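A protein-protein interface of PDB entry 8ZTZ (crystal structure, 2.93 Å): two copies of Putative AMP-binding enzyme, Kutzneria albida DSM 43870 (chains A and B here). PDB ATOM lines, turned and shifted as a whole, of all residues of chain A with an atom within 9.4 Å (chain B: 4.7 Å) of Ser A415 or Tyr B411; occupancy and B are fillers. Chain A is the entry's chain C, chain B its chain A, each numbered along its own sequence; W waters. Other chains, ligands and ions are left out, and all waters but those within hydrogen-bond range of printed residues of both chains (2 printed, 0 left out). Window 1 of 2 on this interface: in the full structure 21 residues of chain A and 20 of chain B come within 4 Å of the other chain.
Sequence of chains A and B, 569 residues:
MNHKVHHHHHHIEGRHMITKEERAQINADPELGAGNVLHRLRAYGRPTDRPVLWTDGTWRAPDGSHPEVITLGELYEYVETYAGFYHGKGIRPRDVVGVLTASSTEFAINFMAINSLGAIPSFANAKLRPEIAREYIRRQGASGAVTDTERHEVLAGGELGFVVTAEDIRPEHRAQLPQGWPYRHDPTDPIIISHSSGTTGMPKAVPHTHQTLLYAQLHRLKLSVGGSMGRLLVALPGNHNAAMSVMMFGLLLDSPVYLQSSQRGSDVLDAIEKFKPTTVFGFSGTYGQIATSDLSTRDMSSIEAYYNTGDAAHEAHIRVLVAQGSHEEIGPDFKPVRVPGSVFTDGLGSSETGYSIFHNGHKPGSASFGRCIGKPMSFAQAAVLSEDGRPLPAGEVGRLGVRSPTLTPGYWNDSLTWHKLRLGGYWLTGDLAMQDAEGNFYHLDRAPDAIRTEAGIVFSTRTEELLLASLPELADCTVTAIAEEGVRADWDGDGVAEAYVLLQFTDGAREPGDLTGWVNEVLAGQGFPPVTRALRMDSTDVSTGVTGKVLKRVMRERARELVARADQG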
ATOM      1  N   ALA A 205      -4.046 -22.946  19.391  1.00  0.00           N
ATOM      2  CA  ALA A 205      -3.325 -23.305  20.607  1.00  0.00           C
ATOM      3  C   ALA A 205      -4.307 -23.872  21.636  1.00  0.00           C
ATOM      4  O   ALA A 205      -5.242 -23.183  22.068  1.00  0.00           O
ATOM      5  CB  ALA A 205      -2.574 -22.092  21.156  1.00  0.00           C
ATOM      6  N   PRO A 409      -9.878 -25.859  28.665  1.00  0.00           N
ATOM      7  CA  PRO A 409     -10.744 -24.716  28.985  1.00  0.00           C
ATOM      8  C   PRO A 409     -10.975 -23.741  27.841  1.00  0.00           C
ATOM      9  O   PRO A 409     -11.629 -22.719  28.071  1.00  0.00           O
ATOM     10  CB  PRO A 409      -9.992 -24.028  30.131  1.00  0.00           C
ATOM     11  CG  PRO A 409      -8.630 -24.470  30.000  1.00  0.00           C
ATOM     12  CD  PRO A 409      -8.643 -25.843  29.450  1.00  0.00           C
ATOM     13  N   GLY A 410     -10.470 -24.018  26.629  1.00  0.00           N
ATOM     14  CA  GLY A 410     -10.628 -23.122  25.490  1.00  0.00           C
ATOM     15  C   GLY A 410      -9.337 -22.571  24.901  1.00  0.00           C
ATOM     16  O   GLY A 410      -8.363 -22.335  25.631  1.00  0.00           O
ATOM     17  N   TYR A 411      -9.326 -22.313  23.590  1.00  0.00           N
ATOM     18  CA  TYR A 411      -8.082 -21.992  22.904  1.00  0.00           C
ATOM     19  C   TYR A 411      -7.447 -20.735  23.472  1.00  0.00           C
ATOM     20  O   TYR A 411      -8.116 -19.838  23.992  1.00  0.00           O
ATOM     21  CB  TYR A 411      -8.303 -21.814  21.416  1.00  0.00           C
ATOM     22  CG  TYR A 411      -9.026 -22.947  20.774  1.00  0.00           C
ATOM     23  CD1 TYR A 411      -8.426 -24.199  20.642  1.00  0.00           C
ATOM     24  CD2 TYR A 411     -10.319 -22.776  20.287  1.00  0.00           C
ATOM     25  CE1 TYR A 411      -9.096 -25.255  20.048  1.00  0.00           C
ATOM     26  CE2 TYR A 411     -11.003 -23.822  19.685  1.00  0.00           C
ATOM     27  CZ  TYR A 411     -10.388 -25.060  19.567  1.00  0.00           C
ATOM     28  OH  TYR A 411     -11.077 -26.094  18.966  1.00  0.00           O
ATOM     29  N   TRP A 412      -6.133 -20.677  23.352  1.00  0.00           N
ATOM     30  CA  TRP A 412      -5.337 -19.689  24.058  1.00  0.00           C
ATOM     31  C   TRP A 412      -5.378 -18.361  23.320  1.00  0.00           C
ATOM     32  O   TRP A 412      -4.868 -18.253  22.196  1.00  0.00           O
ATOM     33  CB  TRP A 412      -3.903 -20.191  24.190  1.00  0.00           C
ATOM     34  CG  TRP A 412      -3.058 -19.327  25.052  1.00  0.00           C
ATOM     35  CD1 TRP A 412      -2.196 -18.344  24.643  1.00  0.00           C
ATOM     36  CD2 TRP A 412      -2.987 -19.357  26.487  1.00  0.00           C
ATOM     37  NE1 TRP A 412      -1.595 -17.764  25.738  1.00  0.00           N
ATOM     38  CE2 TRP A 412      -2.057 -18.370  26.879  1.00  0.00           C
ATOM     39  CE3 TRP A 412      -3.608 -20.127  27.469  1.00  0.00           C
ATOM     40  CZ2 TRP A 412      -1.739 -18.129  28.212  1.00  0.00           C
ATOM     41  CZ3 TRP A 412      -3.300 -19.881  28.786  1.00  0.00           C
ATOM     42  CH2 TRP A 412      -2.369 -18.890  29.147  1.00  0.00           C
ATOM     43  N   ASN A 413      -5.954 -17.348  23.969  1.00  0.00           N
ATOM     44  CA  ASN A 413      -6.073 -15.988  23.446  1.00  0.00           C
ATOM     45  C   ASN A 413      -7.020 -15.899  22.256  1.00  0.00           C
ATOM     46  O   ASN A 413      -6.946 -14.949  21.478  1.00  0.00           O
ATOM     47  CB  ASN A 413      -4.706 -15.398  23.069  1.00  0.00           C
ATOM     48  CG  ASN A 413      -3.925 -14.935  24.268  1.00  0.00           C
ATOM     49  OD1 ASN A 413      -4.475 -14.786  25.345  1.00  0.00           O
ATOM     50  ND2 ASN A 413      -2.636 -14.686  24.082  1.00  0.00           N
ATOM     51  N   ASP A 414      -7.911 -16.875  22.095  1.00  0.00           N
ATOM     52  CA  ASP A 414      -8.841 -16.902  20.983  1.00  0.00           C
ATOM     53  C   ASP A 414     -10.210 -17.407  21.472  1.00  0.00           C
ATOM     54  O   ASP A 414     -10.744 -18.439  21.062  1.00  0.00           O
ATOM     55  CB  ASP A 414      -8.261 -17.733  19.850  1.00  0.00           C
ATOM     56  CG  ASP A 414      -9.053 -17.578  18.577  1.00  0.00           C
ATOM     57  OD1 ASP A 414     -10.018 -16.766  18.555  1.00  0.00           O
ATOM     58  OD2 ASP A 414      -8.710 -18.279  17.599  1.00  0.00           O
ATOM     59  N   SER A 415     -10.785 -16.654  22.407  1.00  0.00           N
ATOM     60  CA  SER A 415     -12.156 -16.882  22.839  1.00  0.00           C
ATOM     61  C   SER A 415     -13.124 -16.985  21.664  1.00  0.00           C
ATOM     62  O   SER A 415     -14.090 -17.759  21.717  1.00  0.00           O
ATOM     63  CB  SER A 415     -12.576 -15.739  23.765  1.00  0.00           C
ATOM     64  OG  SER A 415     -11.678 -15.616  24.844  1.00  0.00           O
ATOM     65  N   LEU A 416     -12.893 -16.198  20.603  1.00  0.00           N
ATOM     66  CA  LEU A 416     -13.834 -16.110  19.486  1.00  0.00           C
ATOM     67  C   LEU A 416     -13.966 -17.442  18.766  1.00  0.00           C
ATOM     68  O   LEU A 416     -15.078 -17.932  18.538  1.00  0.00           O
ATOM     69  CB  LEU A 416     -13.392 -15.031  18.504  1.00  0.00           C
ATOM     70  CG  LEU A 416     -14.371 -14.807  17.374  1.00  0.00           C
ATOM     71  CD1 LEU A 416     -15.709 -14.481  17.952  1.00  0.00           C
ATOM     72  CD2 LEU A 416     -13.898 -13.683  16.540  1.00  0.00           C
ATOM     73  N   THR A 417     -12.837 -18.040  18.387  1.00  0.00           N
ATOM     74  CA  THR A 417     -12.918 -19.356  17.783  1.00  0.00           C
ATOM     75  C   THR A 417     -13.485 -20.369  18.767  1.00  0.00           C
ATOM     76  O   THR A 417     -14.317 -21.197  18.386  1.00  0.00           O
ATOM     77  CB  THR A 417     -11.546 -19.788  17.276  1.00  0.00           C
ATOM     78  OG1 THR A 417     -11.134 -18.906  16.230  1.00  0.00           O
ATOM     79  CG2 THR A 417     -11.591 -21.224  16.736  1.00  0.00           C
ATOM     80  N   TRP A 418     -13.069 -20.300  20.043  1.00  0.00           N
ATOM     81  CA  TRP A 418     -13.470 -21.301  21.025  1.00  0.00           C
ATOM     82  C   TRP A 418     -14.984 -21.435  21.086  1.00  0.00           C
ATOM     83  O   TRP A 418     -15.527 -22.547  21.046  1.00  0.00           O
ATOM     84  CB  TRP A 418     -12.909 -20.937  22.397  1.00  0.00           C
ATOM     85  CG  TRP A 418     -13.405 -21.821  23.558  1.00  0.00           C
ATOM     86  CD1 TRP A 418     -14.050 -21.408  24.699  1.00  0.00           C
ATOM     87  CD2 TRP A 418     -13.306 -23.249  23.659  1.00  0.00           C
ATOM     88  NE1 TRP A 418     -14.345 -22.487  25.498  1.00  0.00           N
ATOM     89  CE2 TRP A 418     -13.903 -23.626  24.887  1.00  0.00           C
ATOM     90  CE3 TRP A 418     -12.778 -24.247  22.826  1.00  0.00           C
ATOM     91  CZ2 TRP A 418     -13.982 -24.944  25.301  1.00  0.00           C
ATOM     92  CZ3 TRP A 418     -12.852 -25.564  23.243  1.00  0.00           C
ATOM     93  CH2 TRP A 418     -13.442 -25.903  24.476  1.00  0.00           C
ATOM     94  N   HIS A 419     -15.690 -20.313  21.159  1.00  0.00           N
ATOM     95  CA  HIS A 419     -17.132 -20.405  21.235  1.00  0.00           C
ATOM     96  C   HIS A 419     -17.777 -20.628  19.881  1.00  0.00           C
ATOM     97  O   HIS A 419     -18.919 -21.096  19.824  1.00  0.00           O
ATOM     98  CB  HIS A 419     -17.685 -19.163  21.887  1.00  0.00           C
ATOM     99  CG  HIS A 419     -17.372 -19.089  23.335  1.00  0.00           C
ATOM    100  ND1 HIS A 419     -17.992 -19.897  24.258  1.00  0.00           N
ATOM    101  CD2 HIS A 419     -16.495 -18.322  24.025  1.00  0.00           C
ATOM    102  CE1 HIS A 419     -17.513 -19.631  25.459  1.00  0.00           C
ATOM    103  NE2 HIS A 419     -16.610 -18.674  25.345  1.00  0.00           N
ATOM    104  N   LYS A 420     -17.078 -20.318  18.794  1.00  0.00           N
ATOM    105  CA  LYS A 420     -17.563 -20.733  17.487  1.00  0.00           C
ATOM    106  C   LYS A 420     -17.578 -22.246  17.367  1.00  0.00           C
ATOM    107  O   LYS A 420     -18.316 -22.783  16.532  1.00  0.00           O
ATOM    108  CB  LYS A 420     -16.713 -20.120  16.374  1.00  0.00           C
ATOM    109  CG  LYS A 420     -16.948 -18.643  16.171  1.00  0.00           C
ATOM    110  CD  LYS A 420     -16.358 -18.132  14.895  1.00  0.00           C
ATOM    111  CE  LYS A 420     -16.553 -16.631  14.827  1.00  0.00           C
ATOM    112  NZ  LYS A 420     -15.901 -16.009  13.637  1.00  0.00           N
ATOM    113  N   LEU A 421     -16.818 -22.946  18.209  1.00  0.00           N
ATOM    114  CA  LEU A 421     -16.712 -24.396  18.137  1.00  0.00           C
ATOM    115  C   LEU A 421     -17.497 -25.087  19.232  1.00  0.00           C
ATOM    116  O   LEU A 421     -17.250 -26.268  19.512  1.00  0.00           O
ATOM    117  CB  LEU A 421     -15.250 -24.832  18.180  1.00  0.00           C
ATOM    118  CG  LEU A 421     -14.703 -24.988  16.765  1.00  0.00           C
ATOM    119  CD1 LEU A 421     -13.216 -24.785  16.780  1.00  0.00           C
ATOM    120  CD2 LEU A 421     -15.019 -26.375  16.274  1.00  0.00           C
ATOM    121  N   ARG A 422     -18.447 -24.389  19.840  1.00  0.00           N
ATOM    122  CA  ARG A 422     -19.232 -24.960  20.915  1.00  0.00           C
ATOM    123  C   ARG A 422     -20.710 -24.883  20.566  1.00  0.00           C
ATOM    124  O   ARG A 422     -21.143 -23.997  19.823  1.00  0.00           O
ATOM    125  CB  ARG A 422     -18.934 -24.258  22.217  1.00  0.00           C
ATOM    126  CG  ARG A 422     -17.624 -24.687  22.820  1.00  0.00           C
ATOM    127  CD  ARG A 422     -17.223 -23.829  24.026  1.00  0.00           C
ATOM    128  NE  ARG A 422     -18.376 -23.491  24.854  1.00  0.00           N
ATOM    129  CZ  ARG A 422     -18.803 -24.219  25.869  1.00  0.00           C
ATOM    130  NH1 ARG A 422     -18.154 -25.305  26.258  1.00  0.00           N
ATOM    131  NH2 ARG A 422     -19.911 -23.855  26.499  1.00  0.00           N
ATOM    132  N   LYS B 204      -9.625  -4.478  30.047  1.00  0.00           N
ATOM    133  CA  LYS B 204      -9.820  -5.911  29.860  1.00  0.00           C
ATOM    134  C   LYS B 204     -11.277  -6.168  29.499  1.00  0.00           C
ATOM    135  O   LYS B 204     -12.185  -5.605  30.111  1.00  0.00           O
ATOM    136  CB  LYS B 204      -9.427  -6.677  31.123  1.00  0.00           C
ATOM    137  CG  LYS B 204      -8.031  -6.289  31.666  1.00  0.00           C
ATOM    138  CD  LYS B 204      -7.512  -7.234  32.733  1.00  0.00           C
ATOM    139  CE  LYS B 204      -7.464  -6.547  34.070  1.00  0.00           C
ATOM    140  NZ  LYS B 204      -8.779  -6.581  34.774  1.00  0.00           N
ATOM    141  N   ALA B 205     -11.503  -6.988  28.487  1.00  0.00           N
ATOM    142  CA  ALA B 205     -12.848  -7.289  28.017  1.00  0.00           C
ATOM    143  C   ALA B 205     -13.400  -8.514  28.756  1.00  0.00           C
ATOM    144  O   ALA B 205     -12.844  -9.613  28.641  1.00  0.00           O
ATOM    145  CB  ALA B 205     -12.812  -7.536  26.515  1.00  0.00           C
ATOM    146  N   VAL B 206     -14.495  -8.346  29.485  1.00  0.00           N
ATOM    147  CA  VAL B 206     -14.984  -9.397  30.374  1.00  0.00           C
ATOM    148  C   VAL B 206     -16.263  -9.997  29.796  1.00  0.00           C
ATOM    149  O   VAL B 206     -17.273  -9.293  29.695  1.00  0.00           O
ATOM    150  CB  VAL B 206     -15.230  -8.859  31.788  1.00  0.00           C
ATOM    151  CG1 VAL B 206     -15.607 -10.008  32.737  1.00  0.00           C
ATOM    152  CG2 VAL B 206     -14.003  -8.114  32.253  1.00  0.00           C
ATOM    153  N   PRO B 207     -16.279 -11.278  29.424  1.00  0.00           N
ATOM    154  CA  PRO B 207     -17.515 -11.898  28.935  1.00  0.00           C
ATOM    155  C   PRO B 207     -18.335 -12.501  30.066  1.00  0.00           C
ATOM    156  O   PRO B 207     -17.805 -12.920  31.094  1.00  0.00           O
ATOM    157  CB  PRO B 207     -16.992 -12.999  28.003  1.00  0.00           C
ATOM    158  CG  PRO B 207     -15.709 -13.411  28.631  1.00  0.00           C
ATOM    159  CD  PRO B 207     -15.124 -12.182  29.275  1.00  0.00           C
ATOM    160  N   GLU B 352     -15.978  -8.543  36.611  1.00  0.00           N
ATOM    161  CA  GLU B 352     -15.609  -9.940  36.526  1.00  0.00           C
ATOM    162  C   GLU B 352     -16.554 -10.838  37.325  1.00  0.00           C
ATOM    163  O   GLU B 352     -16.685 -12.021  36.995  1.00  0.00           O
ATOM    164  CB  GLU B 352     -14.154 -10.093  36.983  1.00  0.00           C
ATOM    165  CG  GLU B 352     -13.093  -9.683  35.951  1.00  0.00           C
ATOM    166  CD  GLU B 352     -12.630  -8.230  36.097  1.00  0.00           C
ATOM    167  OE1 GLU B 352     -13.426  -7.386  36.561  1.00  0.00           O
ATOM    168  OE2 GLU B 352     -11.464  -7.921  35.754  1.00  0.00           O
ATOM    169  N   GLY B 410     -13.423 -15.789  31.824  1.00  0.00           N
ATOM    170  CA  GLY B 410     -12.104 -15.350  31.417  1.00  0.00           C
ATOM    171  C   GLY B 410     -12.074 -14.262  30.366  1.00  0.00           C
ATOM    172  O   GLY B 410     -12.895 -14.265  29.434  1.00  0.00           O
ATOM    173  N   TYR B 411     -11.112 -13.336  30.502  1.00  0.00           N
ATOM    174  CA  TYR B 411     -11.032 -12.163  29.638  1.00  0.00           C
ATOM    175  C   TYR B 411     -11.032 -12.572  28.176  1.00  0.00           C
ATOM    176  O   TYR B 411     -10.364 -13.536  27.782  1.00  0.00           O
ATOM    177  CB  TYR B 411      -9.769 -11.379  29.949  1.00  0.00           C
ATOM    178  CG  TYR B 411      -9.705 -10.886  31.361  1.00  0.00           C
ATOM    179  CD1 TYR B 411     -10.753 -10.167  31.910  1.00  0.00           C
ATOM    180  CD2 TYR B 411      -8.604 -11.138  32.148  1.00  0.00           C
ATOM    181  CE1 TYR B 411     -10.699  -9.695  33.194  1.00  0.00           C
ATOM    182  CE2 TYR B 411      -8.548 -10.674  33.430  1.00  0.00           C
ATOM    183  CZ  TYR B 411      -9.602  -9.954  33.948  1.00  0.00           C
ATOM    184  OH  TYR B 411      -9.546  -9.491  35.233  1.00  0.00           O
ATOM    185  N   TRP B 412     -11.802 -11.825  27.377  1.00  0.00           N
ATOM    186  CA  TRP B 412     -12.084 -12.210  26.000  1.00  0.00           C
ATOM    187  C   TRP B 412     -10.831 -12.068  25.156  1.00  0.00           C
ATOM    188  O   TRP B 412     -10.217 -11.000  25.088  1.00  0.00           O
ATOM    189  CB  TRP B 412     -13.225 -11.374  25.433  1.00  0.00           C
ATOM    190  CG  TRP B 412     -13.672 -11.842  24.069  1.00  0.00           C
ATOM    191  CD1 TRP B 412     -13.236 -11.370  22.865  1.00  0.00           C
ATOM    192  CD2 TRP B 412     -14.645 -12.856  23.768  1.00  0.00           C
ATOM    193  NE1 TRP B 412     -13.867 -12.024  21.840  1.00  0.00           N
ATOM    194  CE2 TRP B 412     -14.741 -12.937  22.364  1.00  0.00           C
ATOM    195  CE3 TRP B 412     -15.466 -13.667  24.543  1.00  0.00           C
ATOM    196  CZ2 TRP B 412     -15.611 -13.816  21.718  1.00  0.00           C
ATOM    197  CZ3 TRP B 412     -16.323 -14.550  23.896  1.00  0.00           C
ATOM    198  CH2 TRP B 412     -16.388 -14.619  22.498  1.00  0.00           C
ATOM    199  N   ASN B 413     -10.440 -13.161  24.531  1.00  0.00           N
ATOM    200  CA  ASN B 413      -9.259 -13.229  23.692  1.00  0.00           C
ATOM    201  C   ASN B 413      -7.975 -12.944  24.447  1.00  0.00           C
ATOM    202  O   ASN B 413      -6.937 -12.795  23.820  1.00  0.00           O
ATOM    203  CB  ASN B 413      -9.398 -12.297  22.496  1.00  0.00           C
ATOM    204  CG  ASN B 413     -10.275 -12.887  21.433  1.00  0.00           C
ATOM    205  OD1 ASN B 413     -10.423 -14.098  21.387  1.00  0.00           O
ATOM    206  ND2 ASN B 413     -10.852 -12.054  20.562  1.00  0.00           N
ATOM    207  N   ASP B 414      -7.982 -12.896  25.776  1.00  0.00           N
ATOM    208  CA  ASP B 414      -6.737 -12.710  26.519  1.00  0.00           C
ATOM    209  C   ASP B 414      -6.640 -13.758  27.617  1.00  0.00           C
ATOM    210  O   ASP B 414      -6.875 -13.467  28.790  1.00  0.00           O
ATOM    211  CB  ASP B 414      -6.632 -11.300  27.072  1.00  0.00           C
ATOM    212  CG  ASP B 414      -5.213 -10.961  27.544  1.00  0.00           C
ATOM    213  OD1 ASP B 414      -4.284 -11.803  27.391  1.00  0.00           O
ATOM    214  OD2 ASP B 414      -5.042  -9.846  28.073  1.00  0.00           O
ATOM    215  N   SER B 415      -6.265 -14.974  27.219  1.00  0.00           N
ATOM    216  CA  SER B 415      -5.973 -16.043  28.171  1.00  0.00           C
ATOM    217  C   SER B 415      -4.832 -15.680  29.115  1.00  0.00           C
ATOM    218  O   SER B 415      -4.911 -15.925  30.328  1.00  0.00           O
ATOM    219  CB  SER B 415      -5.618 -17.308  27.405  1.00  0.00           C
ATOM    220  OG  SER B 415      -6.740 -17.766  26.683  1.00  0.00           O
ATOM    221  N   THR B 417      -3.620 -12.915  30.378  1.00  0.00           N
ATOM    222  CA  THR B 417      -3.874 -12.031  31.504  1.00  0.00           C
ATOM    223  C   THR B 417      -4.845 -12.669  32.477  1.00  0.00           C
ATOM    224  O   THR B 417      -4.739 -12.479  33.694  1.00  0.00           O
ATOM    225  CB  THR B 417      -4.422 -10.700  31.022  1.00  0.00           C
ATOM    226  OG1 THR B 417      -3.515 -10.129  30.089  1.00  0.00           O
ATOM    227  CG2 THR B 417      -4.587  -9.745  32.190  1.00  0.00           C
ATOM    228  N   TRP B 418      -5.822 -13.404  31.953  1.00  0.00           N
ATOM    229  CA  TRP B 418      -6.736 -14.138  32.809  1.00  0.00           C
ATOM    230  C   TRP B 418      -5.964 -14.921  33.860  1.00  0.00           C
ATOM    231  O   TRP B 418      -6.125 -14.695  35.066  1.00  0.00           O
ATOM    232  CB  TRP B 418      -7.591 -15.056  31.941  1.00  0.00           C
ATOM    233  CG  TRP B 418      -8.545 -15.925  32.672  1.00  0.00           C
ATOM    234  CD1 TRP B 418      -8.648 -17.272  32.570  1.00  0.00           C
ATOM    235  CD2 TRP B 418      -9.549 -15.512  33.607  1.00  0.00           C
ATOM    236  NE1 TRP B 418      -9.670 -17.734  33.373  1.00  0.00           N
ATOM    237  CE2 TRP B 418     -10.236 -16.668  34.020  1.00  0.00           C
ATOM    238  CE3 TRP B 418      -9.938 -14.280  34.132  1.00  0.00           C
ATOM    239  CZ2 TRP B 418     -11.272 -16.631  34.928  1.00  0.00           C
ATOM    240  CZ3 TRP B 418     -10.984 -14.253  35.032  1.00  0.00           C
ATOM    241  CH2 TRP B 418     -11.631 -15.418  35.418  1.00  0.00           C
ATOM    242  N   LEU B 421      -3.957 -13.242  36.594  1.00  0.00           N
ATOM    243  CA  LEU B 421      -4.829 -12.783  37.674  1.00  0.00           C
ATOM    244  C   LEU B 421      -5.645 -13.909  38.302  1.00  0.00           C
ATOM    245  O   LEU B 421      -6.753 -13.654  38.785  1.00  0.00           O
ATOM    246  CB  LEU B 421      -5.763 -11.680  37.175  1.00  0.00           C
ATOM    247  CG  LEU B 421      -5.049 -10.480  36.578  1.00  0.00           C
ATOM    248  CD1 LEU B 421      -6.061  -9.458  36.099  1.00  0.00           C
ATOM    249  CD2 LEU B 421      -4.177  -9.942  37.643  1.00  0.00           C
ATOM    250  N   TRP B 427      -9.915 -16.094  41.446  1.00  0.00           N
ATOM    251  CA  TRP B 427      -9.632 -14.874  40.724  1.00  0.00           C
ATOM    252  C   TRP B 427      -9.131 -13.843  41.728  1.00  0.00           C
ATOM    253  O   TRP B 427      -9.541 -13.851  42.892  1.00  0.00           O
ATOM    254  CB  TRP B 427     -10.882 -14.365  40.008  1.00  0.00           C
ATOM    255  CG  TRP B 427     -10.645 -13.101  39.311  1.00  0.00           C
ATOM    256  CD1 TRP B 427      -9.792 -12.891  38.267  1.00  0.00           C
ATOM    257  CD2 TRP B 427     -11.232 -11.832  39.615  1.00  0.00           C
ATOM    258  NE1 TRP B 427      -9.821 -11.566  37.891  1.00  0.00           N
ATOM    259  CE2 TRP B 427     -10.702 -10.897  38.703  1.00  0.00           C
ATOM    260  CE3 TRP B 427     -12.156 -11.395  40.560  1.00  0.00           C
ATOM    261  CZ2 TRP B 427     -11.065  -9.555  38.717  1.00  0.00           C
ATOM    262  CZ3 TRP B 427     -12.527 -10.054  40.556  1.00  0.00           C
ATOM    263  CH2 TRP B 427     -11.979  -9.155  39.641  1.00  0.00           C
HETATM  264  O   HOH W   1      -8.935 -16.299  25.839  1.00  0.00           O
HETATM  265  O   HOH W   2      -2.398 -11.850  25.437  1.00  0.00           O
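The side-chain amide oxygen (OD1) of Asn A413 sits at hydrogen-bond distance from the backbone NH (N) of Ser B415 (2.6 Å). The backbone carbonyl oxygen of Asn A413 sits close to the backbone carbonyl oxygen of Asn B413 (3.2 Å). The backbone NH (N) of Asn B413 is in hydrogen-bond range of the side-chain hydroxyl (OG) of Ser A415 (2.8 Å). OD1 of Asn B413 sits at hydrogen-bond distance from N of Leu A416, at 3.3 Å.
The side-chain amino group (NZ) of Lys B204 sits at hydrogen-bond distance from the side-chain hydroxyl (OH) of Tyr B411. OE2 of Glu B352 lies within hydrogen-bond range of OH of Tyr B411, 2.5 Å away. The side-chain carboxylate (OD2) of Asp B414 sits at hydrogen-bond distance from the side-chain hydroxyl (OG1) of Thr B417 (2.5 Å). The side-chain carboxylate of Asp A414 lies within hydrogen-bond range of the side-chain hydroxyl of Thr A417 (2.9 Å). The backbone carbonyl oxygen of Ala B205 sits at hydrogen-bond distance from the backbone NH of Trp B412 (2.8 Å). NE1 of Trp B412 lies close to ND2 of Asn B413 (3.3 Å).
Tyr A411 touches Ser B415 (O to OG, 3.7 Å). Trp A412 touches Ser B415 (CD2 to CB, 3.5 Å). Asn A413 touches Asp B414 (OD1 to CA, 3.3 Å). CA of Asp A414 touches OD1 of Asn B413, 3.2 Å away. Ser A415 touches Tyr B411. Ser A415 touches Trp B412. Trp B412 touches Leu A416. His A419 touches Trp B412 (CD2 to CZ3, 3.8 Å).
Tyr B411 touches just one residue of chain A: Ser A415. Trp B412 touches just these residues of chain A: Ser A415 (3.5 Å), Leu A416 (3.7 Å) and His A419 (3.8 Å). Asn B413 touches four residues of chain A. Of the printed residues of chain B, Asp A414 touches Asn B413. Of the printed residues of chain A, Asp B414 touches Asn A413 (3.3 Å). Printed residues of chain B within 4 Å of Trp A412: Ser B415 (3.5 Å). The nearest printed residue of chain B that does not touch Ser A415 is Asp B414 (4.7 Å). The nearest printed residue of chain A that does not touch Asp B414 is Ser A415 (4.7 Å).
Hydrophobic or aromatic side chains of chain A that line the printed part of chain B: Trp A412, Leu A416 and His A419. Of the 15 printed residues of chain B, 5 touch a printed residue of chain A. Hydrophobic or aromatic side chains of chain B that line the printed part of chain A: Trp B412. Among the printed residues, 12 pairs touch across the chains. Among the printed residues, no Asp or Glu carboxylate lies within 4 Å of a Lys or Arg side-chain nitrogen of the other chain.
Tyr A411 touches Ser B415, and with the chains exchanged Ser A415 touches Tyr B411. Trp A412 touches Ser B415, and with the chains exchanged Ser A415 touches Trp B412. Asn B413 touches its own counterpart, Asn A413. Asn A413 touches Asp B414, and with the chains exchanged Asp A414 touches Asn B413. Of the 12 pairs that touch across the chains among the printed residues, 9 have their exchanged pair printed and touching as well.
Water W2 lies within hydrogen-bond range of the side-chain carboxylate (OD1) of Asp B414 and the side-chain amide nitrogen (ND2) of Asn A413. Water W1 bridges OG of Ser B415 (2.8 Å) and OG of Ser A415 (3.0 Å).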
